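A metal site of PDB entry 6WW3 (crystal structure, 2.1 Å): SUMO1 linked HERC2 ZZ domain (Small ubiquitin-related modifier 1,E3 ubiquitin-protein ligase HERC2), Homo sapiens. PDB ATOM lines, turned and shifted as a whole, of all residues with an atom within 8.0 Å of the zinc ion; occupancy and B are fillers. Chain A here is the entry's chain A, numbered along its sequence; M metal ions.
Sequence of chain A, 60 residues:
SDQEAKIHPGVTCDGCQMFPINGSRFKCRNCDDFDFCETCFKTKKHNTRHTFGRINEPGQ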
ATOM      1  N   THR A  12     -25.922  18.334  16.911  1.00  0.00           N
ATOM      2  CA  THR A  12     -26.124  19.279  17.994  1.00  0.00           C
ATOM      3  C   THR A  12     -26.337  20.673  17.393  1.00  0.00           C
ATOM      4  O   THR A  12     -25.664  21.044  16.432  1.00  0.00           O
ATOM      5  CB  THR A  12     -24.904  19.312  18.924  1.00  0.00           C
ATOM      6  OG1 THR A  12     -24.543  17.981  19.326  1.00  0.00           O
ATOM      7  CG2 THR A  12     -25.148  20.151  20.164  1.00  0.00           C
ATOM      8  N   CYS A  13     -27.283  21.439  17.952  1.00  0.00           N
ATOM      9  CA  CYS A  13     -27.379  22.855  17.599  1.00  0.00           C
ATOM     10  C   CYS A  13     -26.308  23.639  18.347  1.00  0.00           C
ATOM     11  O   CYS A  13     -26.264  23.648  19.572  1.00  0.00           O
ATOM     12  CB  CYS A  13     -28.764  23.425  17.930  1.00  0.00           C
ATOM     13  SG  CYS A  13     -28.847  25.250  17.747  1.00  0.00           S
ATOM     14  N   ASP A  14     -25.436  24.305  17.607  1.00  0.00           N
ATOM     15  CA  ASP A  14     -24.370  25.054  18.248  1.00  0.00           C
ATOM     16  C   ASP A  14     -24.849  26.320  18.925  1.00  0.00           C
ATOM     17  O   ASP A  14     -24.062  26.952  19.625  1.00  0.00           O
ATOM     18  CB  ASP A  14     -23.268  25.389  17.242  1.00  0.00           C
ATOM     19  CG  ASP A  14     -22.576  24.148  16.741  1.00  0.00           C
ATOM     20  OD1 ASP A  14     -21.875  23.513  17.544  1.00  0.00           O
ATOM     21  OD2 ASP A  14     -22.723  23.797  15.551  1.00  0.00           O
ATOM     22  N   GLY A  15     -26.108  26.707  18.729  1.00  0.00           N
ATOM     23  CA  GLY A  15     -26.646  27.883  19.372  1.00  0.00           C
ATOM     24  C   GLY A  15     -27.175  27.637  20.769  1.00  0.00           C
ATOM     25  O   GLY A  15     -26.973  28.457  21.658  1.00  0.00           O
ATOM     26  N   CYS A  16     -27.830  26.477  20.976  1.00  0.00           N
ATOM     27  CA  CYS A  16     -28.529  26.188  22.223  1.00  0.00           C
ATOM     28  C   CYS A  16     -28.239  24.805  22.773  1.00  0.00           C
ATOM     29  O   CYS A  16     -28.836  24.418  23.772  1.00  0.00           O
ATOM     30  CB  CYS A  16     -30.045  26.352  22.047  1.00  0.00           C
ATOM     31  SG  CYS A  16     -30.818  25.090  21.011  1.00  0.00           S
ATOM     32  N   GLN A  17     -27.350  24.040  22.119  1.00  0.00           N
ATOM     33  CA  GLN A  17     -26.952  22.693  22.524  1.00  0.00           C
ATOM     34  C   GLN A  17     -28.095  21.688  22.472  1.00  0.00           C
ATOM     35  O   GLN A  17     -27.981  20.604  23.042  1.00  0.00           O
ATOM     36  CB  GLN A  17     -26.330  22.680  23.923  1.00  0.00           C
ATOM     37  CG  GLN A  17     -25.240  23.702  24.137  1.00  0.00           C
ATOM     38  CD  GLN A  17     -24.229  23.733  23.005  1.00  0.00           C
ATOM     39  OE1 GLN A  17     -23.935  24.799  22.458  1.00  0.00           O
ATOM     40  NE2 GLN A  17     -23.703  22.569  22.635  1.00  0.00           N
ATOM     41  N   MET A  18     -29.191  22.004  21.763  1.00  0.00           N
ATOM     42  CA  MET A  18     -30.241  21.008  21.494  1.00  0.00           C
ATOM     43  C   MET A  18     -29.634  19.767  20.855  1.00  0.00           C
ATOM     44  O   MET A  18     -28.806  19.882  19.942  1.00  0.00           O
ATOM     45  CB  MET A  18     -31.309  21.609  20.578  1.00  0.00           C
ATOM     46  CG  MET A  18     -32.387  20.624  20.090  1.00  0.00           C
ATOM     47  SD  MET A  18     -33.411  21.273  18.745  1.00  0.00           S
ATOM     48  CE  MET A  18     -34.236  22.630  19.550  1.00  0.00           C
ATOM     49  N   PHE A  19     -29.997  18.590  21.367  1.00  0.00           N
ATOM     50  CA  PHE A  19     -29.455  17.328  20.835  1.00  0.00           C
ATOM     51  C   PHE A  19     -30.389  16.137  21.058  1.00  0.00           C
ATOM     52  O   PHE A  19     -30.716  15.818  22.201  1.00  0.00           O
ATOM     53  CB  PHE A  19     -28.097  17.008  21.451  1.00  0.00           C
ATOM     54  CG  PHE A  19     -27.505  15.718  20.955  1.00  0.00           C
ATOM     55  CD1 PHE A  19     -26.790  15.691  19.767  1.00  0.00           C
ATOM     56  CD2 PHE A  19     -27.688  14.541  21.645  1.00  0.00           C
ATOM     57  CE1 PHE A  19     -26.253  14.504  19.300  1.00  0.00           C
ATOM     58  CE2 PHE A  19     -27.161  13.354  21.164  1.00  0.00           C
ATOM     59  CZ  PHE A  19     -26.442  13.339  19.993  1.00  0.00           C
ATOM     60  N   ILE A  21     -31.026  17.715  17.112  1.00  0.00           N
ATOM     61  CA  ILE A  21     -31.917  18.750  16.595  1.00  0.00           C
ATOM     62  C   ILE A  21     -33.227  18.099  16.195  1.00  0.00           C
ATOM     63  O   ILE A  21     -33.250  17.084  15.489  1.00  0.00           O
ATOM     64  CB  ILE A  21     -31.276  19.487  15.411  1.00  0.00           C
ATOM     65  CG1 ILE A  21     -30.002  20.237  15.855  1.00  0.00           C
ATOM     66  CG2 ILE A  21     -32.284  20.479  14.772  1.00  0.00           C
ATOM     67  CD1 ILE A  21     -29.459  21.179  14.808  1.00  0.00           C
ATOM     68  N   ASP A  35     -24.111  23.924  13.092  1.00  0.00           N
ATOM     69  CA  ASP A  35     -25.528  23.731  12.836  1.00  0.00           C
ATOM     70  C   ASP A  35     -26.364  24.561  13.793  1.00  0.00           C
ATOM     71  O   ASP A  35     -25.969  24.790  14.936  1.00  0.00           O
ATOM     72  CB  ASP A  35     -25.940  22.257  12.956  1.00  0.00           C
ATOM     73  CG  ASP A  35     -25.133  21.347  12.034  1.00  0.00           C
ATOM     74  OD1 ASP A  35     -24.060  20.864  12.449  1.00  0.00           O
ATOM     75  OD2 ASP A  35     -25.588  21.085  10.904  1.00  0.00           O
ATOM     76  N   PHE A  36     -27.527  25.022  13.308  1.00  0.00           N
ATOM     77  CA  PHE A  36     -28.541  25.713  14.096  1.00  0.00           C
ATOM     78  C   PHE A  36     -29.842  24.946  14.055  1.00  0.00           C
ATOM     79  O   PHE A  36     -30.234  24.449  13.000  1.00  0.00           O
ATOM     80  CB  PHE A  36     -28.831  27.112  13.520  1.00  0.00           C
ATOM     81  CG  PHE A  36     -27.962  28.205  14.048  1.00  0.00           C
ATOM     82  CD1 PHE A  36     -27.463  28.165  15.343  1.00  0.00           C
ATOM     83  CD2 PHE A  36     -27.681  29.310  13.266  1.00  0.00           C
ATOM     84  CE1 PHE A  36     -26.692  29.200  15.828  1.00  0.00           C
ATOM     85  CE2 PHE A  36     -26.899  30.349  13.757  1.00  0.00           C
ATOM     86  CZ  PHE A  36     -26.403  30.296  15.033  1.00  0.00           C
ATOM     87  N   CYS A  37     -30.555  24.889  15.174  1.00  0.00           N
ATOM     88  CA  CYS A  37     -31.974  24.578  15.069  1.00  0.00           C
ATOM     89  C   CYS A  37     -32.697  25.798  14.489  1.00  0.00           C
ATOM     90  O   CYS A  37     -32.106  26.864  14.280  1.00  0.00           O
ATOM     91  CB  CYS A  37     -32.560  24.167  16.411  1.00  0.00           C
ATOM     92  SG  CYS A  37     -32.765  25.539  17.576  1.00  0.00           S
ATOM     93  N   GLU A  38     -33.988  25.652  14.189  1.00  0.00           N
ATOM     94  CA  GLU A  38     -34.667  26.718  13.465  1.00  0.00           C
ATOM     95  C   GLU A  38     -34.805  27.975  14.330  1.00  0.00           C
ATOM     96  O   GLU A  38     -34.596  29.084  13.833  1.00  0.00           O
ATOM     97  CB  GLU A  38     -36.039  26.273  12.955  1.00  0.00           C
ATOM     98  CG  GLU A  38     -36.766  27.370  12.186  1.00  0.00           C
ATOM     99  CD  GLU A  38     -37.959  26.862  11.374  1.00  0.00           C
ATOM    100  OE1 GLU A  38     -38.100  25.633  11.207  1.00  0.00           O
ATOM    101  OE2 GLU A  38     -38.759  27.699  10.933  1.00  0.00           O
ATOM    102  N   THR A  39     -35.158  27.824  15.605  1.00  0.00           N
ATOM    103  CA  THR A  39     -35.251  28.987  16.477  1.00  0.00           C
ATOM    104  C   THR A  39     -33.919  29.731  16.540  1.00  0.00           C
ATOM    105  O   THR A  39     -33.860  30.947  16.372  1.00  0.00           O
ATOM    106  CB  THR A  39     -35.690  28.602  17.885  1.00  0.00           C
ATOM    107  OG1 THR A  39     -36.981  27.978  17.841  1.00  0.00           O
ATOM    108  CG2 THR A  39     -35.770  29.864  18.746  1.00  0.00           C
ATOM    109  N   CYS A  40     -32.823  28.985  16.757  1.00  0.00           N
ATOM    110  CA  CYS A  40     -31.509  29.609  16.786  1.00  0.00           C
ATOM    111  C   CYS A  40     -31.166  30.237  15.443  1.00  0.00           C
ATOM    112  O   CYS A  40     -30.579  31.332  15.403  1.00  0.00           O
ATOM    113  CB  CYS A  40     -30.438  28.578  17.167  1.00  0.00           C
ATOM    114  SG  CYS A  40     -30.427  28.188  18.899  1.00  0.00           S
ATOM    115  N   PHE A  41     -31.521  29.567  14.347  1.00  0.00           N
ATOM    116  CA  PHE A  41     -31.249  30.139  13.026  1.00  0.00           C
ATOM    117  C   PHE A  41     -31.911  31.493  12.862  1.00  0.00           C
ATOM    118  O   PHE A  41     -31.348  32.367  12.188  1.00  0.00           O
ATOM    119  CB  PHE A  41     -31.716  29.196  11.915  1.00  0.00           C
ATOM    120  CG  PHE A  41     -31.627  29.816  10.549  1.00  0.00           C
ATOM    121  CD1 PHE A  41     -30.387  30.142   9.986  1.00  0.00           C
ATOM    122  CD2 PHE A  41     -32.767  30.078   9.815  1.00  0.00           C
ATOM    123  CE1 PHE A  41     -30.290  30.708   8.735  1.00  0.00           C
ATOM    124  CE2 PHE A  41     -32.687  30.652   8.540  1.00  0.00           C
ATOM    125  CZ  PHE A  41     -31.451  30.975   8.008  1.00  0.00           C
ATOM    126  N   THR A  43     -32.657  33.655  15.373  1.00  0.00           N
ATOM    127  CA  THR A  43     -32.445  34.615  16.461  1.00  0.00           C
ATOM    128  C   THR A  43     -30.992  34.844  16.846  1.00  0.00           C
ATOM    129  O   THR A  43     -30.652  35.876  17.427  1.00  0.00           O
ATOM    130  CB  THR A  43     -33.229  34.187  17.714  1.00  0.00           C
ATOM    131  OG1 THR A  43     -32.743  32.928  18.183  1.00  0.00           O
ATOM    132  CG2 THR A  43     -34.704  34.070  17.405  1.00  0.00           C
ATOM    133  N   LYS A  44     -30.133  33.862  16.608  1.00  0.00           N
ATOM    134  CA  LYS A  44     -28.737  33.994  17.013  1.00  0.00           C
ATOM    135  C   LYS A  44     -27.945  34.755  15.962  1.00  0.00           C
ATOM    136  O   LYS A  44     -28.194  34.642  14.766  1.00  0.00           O
ATOM    137  CB  LYS A  44     -28.087  32.634  17.261  1.00  0.00           C
ATOM    138  CG  LYS A  44     -28.063  32.163  18.714  1.00  0.00           C
ATOM    139  CD  LYS A  44     -29.400  31.973  19.318  1.00  0.00           C
ATOM    140  CE  LYS A  44     -29.266  31.141  20.579  1.00  0.00           C
ATOM    141  NZ  LYS A  44     -30.587  31.050  21.254  1.00  0.00           N
HETATM  142 ZN    ZN M   1     -30.753  25.971  18.881  1.00  0.00          ZN
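Within 4 Å of the zinc ion: Cys 13, Cys 16, Cys 37 and Cys 40.
The nearest printed residue that does not touch the zinc ion is Gly 15 (4.4 Å).
The backbone NH of Cys 13 sits at hydrogen-bond distance from the backbone carbonyl oxygen of Met 18, at 3.0 Å.
The side-chain sulfur of Cys 40 lies close to the side-chain amino group of Lys 44, at 3.7 Å.
The backbone NH (N) of Gly 15 sits close to the side-chain sulfur (SG) of Cys 13, 3.3 Å away.
SG of Cys 16 lies close to N of Met 18.
SG of Cys 40 binds the zinc ion, at 2.2 Å.
SG of Cys 16 is bound to the zinc ion (2.3 Å).
The zinc ion is bound by the side-chain sulfur (SG) of Cys 13 (2.3 Å).
SG of Cys 37 binds the zinc ion (2.4 Å).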
